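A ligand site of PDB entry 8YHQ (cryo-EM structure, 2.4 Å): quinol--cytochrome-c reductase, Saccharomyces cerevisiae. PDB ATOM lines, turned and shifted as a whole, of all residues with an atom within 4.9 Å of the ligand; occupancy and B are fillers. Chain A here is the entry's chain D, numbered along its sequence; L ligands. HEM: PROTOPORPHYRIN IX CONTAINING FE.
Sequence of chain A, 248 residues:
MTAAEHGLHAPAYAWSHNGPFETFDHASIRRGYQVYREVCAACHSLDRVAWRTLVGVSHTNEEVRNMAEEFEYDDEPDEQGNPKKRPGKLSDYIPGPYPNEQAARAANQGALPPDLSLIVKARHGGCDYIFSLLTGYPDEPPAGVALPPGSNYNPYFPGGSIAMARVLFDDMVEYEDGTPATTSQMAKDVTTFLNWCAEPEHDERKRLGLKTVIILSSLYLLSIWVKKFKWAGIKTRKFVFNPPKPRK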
ATOM      1  N   VAL A  35      -7.364   3.453 -37.315  1.00  0.00           N
ATOM      2  CA  VAL A  35      -8.052   3.483 -36.024  1.00  0.00           C
ATOM      3  C   VAL A  35      -7.181   2.845 -34.948  1.00  0.00           C
ATOM      4  O   VAL A  35      -7.220   3.253 -33.780  1.00  0.00           O
ATOM      5  CB  VAL A  35      -9.423   2.793 -36.129  1.00  0.00           C
ATOM      6  CG1 VAL A  35     -10.193   2.929 -34.840  1.00  0.00           C
ATOM      7  CG2 VAL A  35     -10.220   3.367 -37.253  1.00  0.00           C
ATOM      8  N   VAL A  39      -6.100   5.267 -31.779  1.00  0.00           N
ATOM      9  CA  VAL A  39      -6.971   5.000 -30.638  1.00  0.00           C
ATOM     10  C   VAL A  39      -6.452   3.848 -29.786  1.00  0.00           C
ATOM     11  O   VAL A  39      -6.321   3.982 -28.564  1.00  0.00           O
ATOM     12  CB  VAL A  39      -8.422   4.731 -31.084  1.00  0.00           C
ATOM     13  CG1 VAL A  39      -9.349   4.610 -29.891  1.00  0.00           C
ATOM     14  CG2 VAL A  39      -8.898   5.832 -32.001  1.00  0.00           C
ATOM     15  N   CYS A  40      -6.151   2.711 -30.404  1.00  0.00           N
ATOM     16  CA  CYS A  40      -5.885   1.482 -29.668  1.00  0.00           C
ATOM     17  C   CYS A  40      -4.459   1.386 -29.152  1.00  0.00           C
ATOM     18  O   CYS A  40      -4.243   0.939 -28.025  1.00  0.00           O
ATOM     19  CB  CYS A  40      -6.113   0.253 -30.554  1.00  0.00           C
ATOM     20  SG  CYS A  40      -7.646   0.121 -31.431  1.00  0.00           S
ATOM     21  N   CYS A  43      -2.510   1.650 -25.511  1.00  0.00           N
ATOM     22  CA  CYS A  43      -2.555   0.680 -24.427  1.00  0.00           C
ATOM     23  C   CYS A  43      -2.619  -0.770 -24.882  1.00  0.00           C
ATOM     24  O   CYS A  43      -2.790  -1.654 -24.023  1.00  0.00           O
ATOM     25  CB  CYS A  43      -3.755   0.980 -23.518  1.00  0.00           C
ATOM     26  SG  CYS A  43      -3.525   2.502 -22.574  1.00  0.00           S
ATOM     27  N   HIS A  44      -2.463  -1.062 -26.175  1.00  0.00           N
ATOM     28  CA  HIS A  44      -2.460  -2.429 -26.691  1.00  0.00           C
ATOM     29  C   HIS A  44      -1.289  -2.659 -27.626  1.00  0.00           C
ATOM     30  O   HIS A  44      -0.938  -1.783 -28.422  1.00  0.00           O
ATOM     31  CB  HIS A  44      -3.747  -2.752 -27.427  1.00  0.00           C
ATOM     32  CG  HIS A  44      -4.971  -2.624 -26.597  1.00  0.00           C
ATOM     33  ND1 HIS A  44      -5.262  -3.489 -25.564  1.00  0.00           N
ATOM     34  CD2 HIS A  44      -5.983  -1.736 -26.639  1.00  0.00           C
ATOM     35  CE1 HIS A  44      -6.410  -3.137 -25.017  1.00  0.00           C
ATOM     36  NE2 HIS A  44      -6.860  -2.078 -25.646  1.00  0.00           N
ATOM     37  N   ASN A 108      -3.060   1.188 -15.784  1.00  0.00           N
ATOM     38  CA  ASN A 108      -4.440   0.787 -16.025  1.00  0.00           C
ATOM     39  C   ASN A 108      -5.096   0.275 -14.755  1.00  0.00           C
ATOM     40  O   ASN A 108      -6.004  -0.569 -14.803  1.00  0.00           O
ATOM     41  CB  ASN A 108      -4.505  -0.269 -17.135  1.00  0.00           C
ATOM     42  CG  ASN A 108      -4.202   0.297 -18.493  1.00  0.00           C
ATOM     43  OD1 ASN A 108      -5.077   0.837 -19.167  1.00  0.00           O
ATOM     44  ND2 ASN A 108      -2.958   0.155 -18.928  1.00  0.00           N
ATOM     45  N   ALA A 111      -5.136  -3.650 -13.924  1.00  0.00           N
ATOM     46  CA  ALA A 111      -5.520  -4.555 -14.986  1.00  0.00           C
ATOM     47  C   ALA A 111      -4.511  -4.513 -16.131  1.00  0.00           C
ATOM     48  O   ALA A 111      -3.839  -3.504 -16.369  1.00  0.00           O
ATOM     49  CB  ALA A 111      -6.910  -4.226 -15.507  1.00  0.00           C
ATOM     50  N   LEU A 112      -4.430  -5.618 -16.855  1.00  0.00           N
ATOM     51  CA  LEU A 112      -3.506  -5.799 -17.960  1.00  0.00           C
ATOM     52  C   LEU A 112      -4.276  -5.890 -19.273  1.00  0.00           C
ATOM     53  O   LEU A 112      -5.081  -6.818 -19.424  1.00  0.00           O
ATOM     54  CB  LEU A 112      -2.684  -7.062 -17.749  1.00  0.00           C
ATOM     55  CG  LEU A 112      -1.584  -7.391 -18.757  1.00  0.00           C
ATOM     56  CD1 LEU A 112      -0.507  -6.353 -18.751  1.00  0.00           C
ATOM     57  CD2 LEU A 112      -1.010  -8.743 -18.449  1.00  0.00           C
ATOM     58  N   PRO A 113      -4.100  -4.974 -20.225  1.00  0.00           N
ATOM     59  CA  PRO A 113      -4.768  -5.138 -21.519  1.00  0.00           C
ATOM     60  C   PRO A 113      -4.057  -6.168 -22.387  1.00  0.00           C
ATOM     61  O   PRO A 113      -2.814  -6.140 -22.477  1.00  0.00           O
ATOM     62  CB  PRO A 113      -4.695  -3.735 -22.130  1.00  0.00           C
ATOM     63  CG  PRO A 113      -3.641  -3.046 -21.427  1.00  0.00           C
ATOM     64  CD  PRO A 113      -3.536  -3.619 -20.088  1.00  0.00           C
ATOM     65  N   PRO A 114      -4.772  -7.094 -23.031  1.00  0.00           N
ATOM     66  CA  PRO A 114      -4.091  -8.165 -23.764  1.00  0.00           C
ATOM     67  C   PRO A 114      -3.576  -7.737 -25.142  1.00  0.00           C
ATOM     68  O   PRO A 114      -3.984  -6.728 -25.718  1.00  0.00           O
ATOM     69  CB  PRO A 114      -5.179  -9.226 -23.916  1.00  0.00           C
ATOM     70  CG  PRO A 114      -6.418  -8.501 -23.879  1.00  0.00           C
ATOM     71  CD  PRO A 114      -6.218  -7.370 -22.944  1.00  0.00           C
ATOM     72  N   LEU A 116      -3.470  -8.175 -29.111  1.00  0.00           N
ATOM     73  CA  LEU A 116      -4.605  -8.291 -30.005  1.00  0.00           C
ATOM     74  C   LEU A 116      -4.293  -9.028 -31.303  1.00  0.00           C
ATOM     75  O   LEU A 116      -5.128  -9.057 -32.200  1.00  0.00           O
ATOM     76  CB  LEU A 116      -5.145  -6.892 -30.318  1.00  0.00           C
ATOM     77  CG  LEU A 116      -5.657  -6.025 -29.172  1.00  0.00           C
ATOM     78  CD1 LEU A 116      -6.129  -4.711 -29.714  1.00  0.00           C
ATOM     79  CD2 LEU A 116      -6.740  -6.710 -28.399  1.00  0.00           C
ATOM     80  N   ILE A 119      -6.774 -12.130 -31.064  1.00  0.00           N
ATOM     81  CA  ILE A 119      -7.969 -11.972 -30.245  1.00  0.00           C
ATOM     82  C   ILE A 119      -9.243 -12.402 -30.964  1.00  0.00           C
ATOM     83  O   ILE A 119     -10.222 -12.744 -30.304  1.00  0.00           O
ATOM     84  CB  ILE A 119      -8.071 -10.523 -29.746  1.00  0.00           C
ATOM     85  CG1 ILE A 119      -8.884 -10.437 -28.472  1.00  0.00           C
ATOM     86  CG2 ILE A 119      -8.649  -9.602 -30.794  1.00  0.00           C
ATOM     87  CD1 ILE A 119      -8.160 -10.862 -27.264  1.00  0.00           C
ATOM     88  N   ARG A 123     -11.518 -16.003 -28.892  1.00  0.00           N
ATOM     89  CA  ARG A 123     -12.749 -15.637 -28.211  1.00  0.00           C
ATOM     90  C   ARG A 123     -13.917 -16.285 -28.930  1.00  0.00           C
ATOM     91  O   ARG A 123     -13.958 -16.328 -30.160  1.00  0.00           O
ATOM     92  CB  ARG A 123     -12.948 -14.114 -28.165  1.00  0.00           C
ATOM     93  CG  ARG A 123     -12.000 -13.351 -27.269  1.00  0.00           C
ATOM     94  CD  ARG A 123     -12.201 -13.682 -25.813  1.00  0.00           C
ATOM     95  NE  ARG A 123     -11.418 -12.835 -24.928  1.00  0.00           N
ATOM     96  CZ  ARG A 123     -10.118 -12.966 -24.692  1.00  0.00           C
ATOM     97  NH1 ARG A 123      -9.534 -12.133 -23.860  1.00  0.00           N
ATOM     98  NH2 ARG A 123      -9.397 -13.904 -25.277  1.00  0.00           N
ATOM     99  N   TYR A 129     -18.339 -10.696 -31.710  1.00  0.00           N
ATOM    100  CA  TYR A 129     -18.177 -10.366 -30.296  1.00  0.00           C
ATOM    101  C   TYR A 129     -17.320  -9.109 -30.125  1.00  0.00           C
ATOM    102  O   TYR A 129     -17.584  -8.287 -29.254  1.00  0.00           O
ATOM    103  CB  TYR A 129     -17.573 -11.544 -29.549  1.00  0.00           C
ATOM    104  CG  TYR A 129     -17.054 -11.203 -28.172  1.00  0.00           C
ATOM    105  CD1 TYR A 129     -17.926 -10.934 -27.133  1.00  0.00           C
ATOM    106  CD2 TYR A 129     -15.695 -11.131 -27.905  1.00  0.00           C
ATOM    107  CE1 TYR A 129     -17.467 -10.608 -25.891  1.00  0.00           C
ATOM    108  CE2 TYR A 129     -15.238 -10.814 -26.666  1.00  0.00           C
ATOM    109  CZ  TYR A 129     -16.124 -10.553 -25.659  1.00  0.00           C
ATOM    110  OH  TYR A 129     -15.671 -10.230 -24.404  1.00  0.00           O
ATOM    111  N   ILE A 130     -16.286  -8.967 -30.956  1.00  0.00           N
ATOM    112  CA  ILE A 130     -15.424  -7.796 -30.883  1.00  0.00           C
ATOM    113  C   ILE A 130     -16.204  -6.530 -31.250  1.00  0.00           C
ATOM    114  O   ILE A 130     -16.086  -5.502 -30.585  1.00  0.00           O
ATOM    115  CB  ILE A 130     -14.189  -7.966 -31.783  1.00  0.00           C
ATOM    116  CG1 ILE A 130     -13.409  -9.261 -31.488  1.00  0.00           C
ATOM    117  CG2 ILE A 130     -13.276  -6.786 -31.646  1.00  0.00           C
ATOM    118  CD1 ILE A 130     -12.602  -9.259 -30.252  1.00  0.00           C
ATOM    119  N   LEU A 133     -18.906  -5.728 -28.529  1.00  0.00           N
ATOM    120  CA  LEU A 133     -18.304  -5.219 -27.312  1.00  0.00           C
ATOM    121  C   LEU A 133     -18.081  -3.709 -27.399  1.00  0.00           C
ATOM    122  O   LEU A 133     -18.514  -2.946 -26.530  1.00  0.00           O
ATOM    123  CB  LEU A 133     -16.986  -5.950 -27.045  1.00  0.00           C
ATOM    124  CG  LEU A 133     -16.284  -5.756 -25.704  1.00  0.00           C
ATOM    125  CD1 LEU A 133     -17.020  -6.454 -24.589  1.00  0.00           C
ATOM    126  CD2 LEU A 133     -14.866  -6.268 -25.815  1.00  0.00           C
ATOM    127  N   LEU A 134     -17.392  -3.270 -28.458  1.00  0.00           N
ATOM    128  CA  LEU A 134     -17.021  -1.863 -28.592  1.00  0.00           C
ATOM    129  C   LEU A 134     -18.227  -0.952 -28.731  1.00  0.00           C
ATOM    130  O   LEU A 134     -18.166   0.219 -28.341  1.00  0.00           O
ATOM    131  CB  LEU A 134     -16.104  -1.706 -29.789  1.00  0.00           C
ATOM    132  CG  LEU A 134     -14.759  -2.419 -29.713  1.00  0.00           C
ATOM    133  CD1 LEU A 134     -14.133  -2.550 -31.081  1.00  0.00           C
ATOM    134  CD2 LEU A 134     -13.804  -1.721 -28.790  1.00  0.00           C
ATOM    135  N   PHE A 157     -19.434  -8.713 -21.910  1.00  0.00           N
ATOM    136  CA  PHE A 157     -18.312  -9.253 -21.174  1.00  0.00           C
ATOM    137  C   PHE A 157     -18.831 -10.188 -20.078  1.00  0.00           C
ATOM    138  O   PHE A 157     -19.796  -9.841 -19.386  1.00  0.00           O
ATOM    139  CB  PHE A 157     -17.499  -8.122 -20.562  1.00  0.00           C
ATOM    140  CG  PHE A 157     -16.145  -8.532 -20.062  1.00  0.00           C
ATOM    141  CD1 PHE A 157     -15.183  -9.005 -20.915  1.00  0.00           C
ATOM    142  CD2 PHE A 157     -15.832  -8.414 -18.723  1.00  0.00           C
ATOM    143  CE1 PHE A 157     -13.953  -9.362 -20.457  1.00  0.00           C
ATOM    144  CE2 PHE A 157     -14.605  -8.780 -18.269  1.00  0.00           C
ATOM    145  CZ  PHE A 157     -13.659  -9.245 -19.135  1.00  0.00           C
ATOM    146  N   ILE A 162     -16.143  -4.665 -16.846  1.00  0.00           N
ATOM    147  CA  ILE A 162     -14.899  -4.718 -17.593  1.00  0.00           C
ATOM    148  C   ILE A 162     -14.066  -3.506 -17.221  1.00  0.00           C
ATOM    149  O   ILE A 162     -14.581  -2.431 -16.906  1.00  0.00           O
ATOM    150  CB  ILE A 162     -15.157  -4.796 -19.111  1.00  0.00           C
ATOM    151  CG1 ILE A 162     -13.895  -5.174 -19.869  1.00  0.00           C
ATOM    152  CG2 ILE A 162     -15.750  -3.507 -19.627  1.00  0.00           C
ATOM    153  CD1 ILE A 162     -14.096  -5.376 -21.315  1.00  0.00           C
ATOM    154  N   ALA A 163     -12.754  -3.688 -17.246  1.00  0.00           N
ATOM    155  CA  ALA A 163     -11.810  -2.653 -16.871  1.00  0.00           C
ATOM    156  C   ALA A 163     -11.619  -1.582 -17.935  1.00  0.00           C
ATOM    157  O   ALA A 163     -11.108  -0.502 -17.630  1.00  0.00           O
ATOM    158  CB  ALA A 163     -10.451  -3.282 -16.552  1.00  0.00           C
ATOM    159  N   MET A 164     -12.010  -1.856 -19.182  1.00  0.00           N
ATOM    160  CA  MET A 164     -11.951  -0.881 -20.258  1.00  0.00           C
ATOM    161  C   MET A 164     -13.173   0.020 -20.207  1.00  0.00           C
ATOM    162  O   MET A 164     -14.290  -0.447 -19.967  1.00  0.00           O
ATOM    163  CB  MET A 164     -11.880  -1.589 -21.608  1.00  0.00           C
ATOM    164  CG  MET A 164     -11.830  -0.672 -22.822  1.00  0.00           C
ATOM    165  SD  MET A 164     -11.683  -1.475 -24.409  1.00  0.00           S
ATOM    166  CE  MET A 164     -13.202  -2.393 -24.543  1.00  0.00           C
ATOM    167  N   VAL A 167     -14.158   3.979 -25.606  1.00  0.00           N
ATOM    168  CA  VAL A 167     -13.085   4.736 -26.238  1.00  0.00           C
ATOM    169  C   VAL A 167     -13.455   5.244 -27.625  1.00  0.00           C
ATOM    170  O   VAL A 167     -12.638   5.950 -28.233  1.00  0.00           O
ATOM    171  CB  VAL A 167     -11.780   3.909 -26.336  1.00  0.00           C
ATOM    172  CG1 VAL A 167     -11.392   3.376 -24.979  1.00  0.00           C
ATOM    173  CG2 VAL A 167     -11.909   2.784 -27.333  1.00  0.00           C
ATOM    174  N   LEU A 168     -14.630   4.910 -28.155  1.00  0.00           N
ATOM    175  CA  LEU A 168     -15.031   5.288 -29.494  1.00  0.00           C
ATOM    176  C   LEU A 168     -16.204   6.265 -29.442  1.00  0.00           C
ATOM    177  O   LEU A 168     -17.131   6.087 -28.637  1.00  0.00           O
ATOM    178  CB  LEU A 168     -15.402   4.063 -30.331  1.00  0.00           C
ATOM    179  CG  LEU A 168     -14.263   3.122 -30.739  1.00  0.00           C
ATOM    180  CD1 LEU A 168     -14.814   1.990 -31.576  1.00  0.00           C
ATOM    181  CD2 LEU A 168     -13.149   3.826 -31.493  1.00  0.00           C
ATOM    182  N   VAL A 190     -11.909  -1.642 -37.569  1.00  0.00           N
ATOM    183  CA  VAL A 190     -10.980  -2.177 -36.576  1.00  0.00           C
ATOM    184  C   VAL A 190     -11.035  -3.701 -36.553  1.00  0.00           C
ATOM    185  O   VAL A 190     -10.005  -4.373 -36.551  1.00  0.00           O
ATOM    186  CB  VAL A 190     -11.286  -1.568 -35.197  1.00  0.00           C
ATOM    187  CG1 VAL A 190     -10.622  -2.305 -34.079  1.00  0.00           C
ATOM    188  CG2 VAL A 190     -10.776  -0.199 -35.160  1.00  0.00           C
ATOM    189  N   LEU A 194      -8.186  -6.531 -37.523  1.00  0.00           N
ATOM    190  CA  LEU A 194      -7.737  -7.475 -36.514  1.00  0.00           C
ATOM    191  C   LEU A 194      -7.908  -8.913 -36.966  1.00  0.00           C
ATOM    192  O   LEU A 194      -7.096  -9.781 -36.611  1.00  0.00           O
ATOM    193  CB  LEU A 194      -8.467  -7.226 -35.202  1.00  0.00           C
ATOM    194  CG  LEU A 194      -8.047  -6.007 -34.377  1.00  0.00           C
ATOM    195  CD1 LEU A 194      -8.924  -5.866 -33.158  1.00  0.00           C
ATOM    196  CD2 LEU A 194      -6.599  -6.072 -33.962  1.00  0.00           C
HETATM  197  CHA HEM L   1      -9.710  -5.146 -23.194  1.00  0.00           C
HETATM  198  CHB HEM L   1      -9.625  -3.942 -27.874  1.00  0.00           C
HETATM  199  CHC HEM L   1      -8.851   0.663 -26.765  1.00  0.00           C
HETATM  200  CHD HEM L   1      -7.870  -0.753 -22.244  1.00  0.00           C
HETATM  201  C1A HEM L   1      -9.880  -5.243 -24.559  1.00  0.00           C
HETATM  202  C2A HEM L   1     -10.432  -6.335 -25.355  1.00  0.00           C
HETATM  203  C3A HEM L   1     -10.404  -5.962 -26.639  1.00  0.00           C
HETATM  204  C4A HEM L   1      -9.830  -4.641 -26.721  1.00  0.00           C
HETATM  205  CMA HEM L   1     -10.887  -6.809 -27.834  1.00  0.00           C
HETATM  206  CAA HEM L   1     -11.015  -7.727 -25.009  1.00  0.00           C
HETATM  207  CBA HEM L   1     -10.789  -8.327 -23.638  1.00  0.00           C
HETATM  208  CGA HEM L   1     -11.955  -9.222 -23.322  1.00  0.00           C
HETATM  209  O1A HEM L   1     -13.095  -8.705 -23.277  1.00  0.00           O
HETATM  210  O2A HEM L   1     -11.757 -10.443 -23.117  1.00  0.00           O
HETATM  211  C1B HEM L   1      -9.586  -2.576 -27.961  1.00  0.00           C
HETATM  212  C2B HEM L   1     -10.055  -1.789 -29.066  1.00  0.00           C
HETATM  213  C3B HEM L   1      -9.835  -0.495 -28.757  1.00  0.00           C
HETATM  214  C4B HEM L   1      -9.234  -0.463 -27.446  1.00  0.00           C
HETATM  215  CMB HEM L   1     -10.655  -2.432 -30.333  1.00  0.00           C
HETATM  216  CAB HEM L   1     -10.138   0.812 -29.536  1.00  0.00           C
HETATM  217  CBB HEM L   1     -10.850   0.835 -30.659  1.00  0.00           C
HETATM  218  C1C HEM L   1      -8.409   0.658 -25.464  1.00  0.00           C
HETATM  219  C2C HEM L   1      -7.787   1.764 -24.784  1.00  0.00           C
HETATM  220  C3C HEM L   1      -7.491   1.376 -23.534  1.00  0.00           C
HETATM  221  C4C HEM L   1      -7.963   0.008 -23.387  1.00  0.00           C
HETATM  222  CMC HEM L   1      -7.491   3.127 -25.480  1.00  0.00           C
HETATM  223  CAC HEM L   1      -6.835   2.156 -22.382  1.00  0.00           C
HETATM  224  CBC HEM L   1      -6.988   3.468 -22.227  1.00  0.00           C
HETATM  225  C1D HEM L   1      -8.295  -2.054 -22.098  1.00  0.00           C
HETATM  226  C2D HEM L   1      -8.237  -2.844 -20.883  1.00  0.00           C
HETATM  227  C3D HEM L   1      -8.745  -4.049 -21.139  1.00  0.00           C
HETATM  228  C4D HEM L   1      -9.132  -4.077 -22.536  1.00  0.00           C
HETATM  229  CMD HEM L   1      -7.676  -2.340 -19.533  1.00  0.00           C
HETATM  230  CAD HEM L   1      -8.871  -5.222 -20.136  1.00  0.00           C
HETATM  231  CBD HEM L   1     -10.316  -5.571 -19.812  1.00  0.00           C
HETATM  232  CGD HEM L   1     -10.384  -6.467 -18.616  1.00  0.00           C
HETATM  233  O1D HEM L   1      -9.557  -7.397 -18.493  1.00  0.00           O
HETATM  234  O2D HEM L   1     -11.288  -6.242 -17.770  1.00  0.00           O
HETATM  235  NA  HEM L   1      -9.524  -4.240 -25.440  1.00  0.00           N
HETATM  236  NB  HEM L   1      -9.094  -1.750 -26.989  1.00  0.00           N
HETATM  237  NC  HEM L   1      -8.513  -0.391 -24.578  1.00  0.00           N
HETATM  238  ND  HEM L   1      -8.855  -2.839 -23.082  1.00  0.00           N
HETATM  239 FE   HEM L   1      -8.988  -2.294 -25.029  1.00  0.00          FE
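NE2 of His 44 binds FE of the ligand (2.2 Å).
An oxygen (O2A) of the ligand is in salt-bridge range of the guanidinium group (NH1) of Arg 123, at 2.9 Å.
An oxygen (O2D) of the ligand lies within hydrogen-bond range of the backbone NH of Ala 163, 3.0 Å away.
OH of Tyr 129 sits at hydrogen-bond distance from O1A of the ligand.
SD of Met 164 sits close to NC of the ligand (3.4 Å).
Merely in contact with the ligand: Val 39 (3.4 Å), Cys 40 (3.2 Å), Cys 43 (3.3 Å), Asn 108 (3.9 Å), Pro 113 (3.9 Å), Ile 130 (3.8 Å), Leu 133 (3.9 Å), Leu 134 (3.6 Å), Phe 157 (3.0 Å), Ile 162 (3.5 Å), Val 167 (3.4 Å), Leu 168 (3.9 Å) and Val 190 (3.7 Å).
Hydrophobic or aromatic side chains that line the ligand: Val 39, His 44, Pro 113, Ile 130, Leu 133, Leu 134, Phe 157, Ile 162, Ala 163, Met 164, Val 167, Leu 168 and Val 190.
ND1 of His 44 is in hydrogen-bond range of O of Pro 114, 3.5 Å away.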
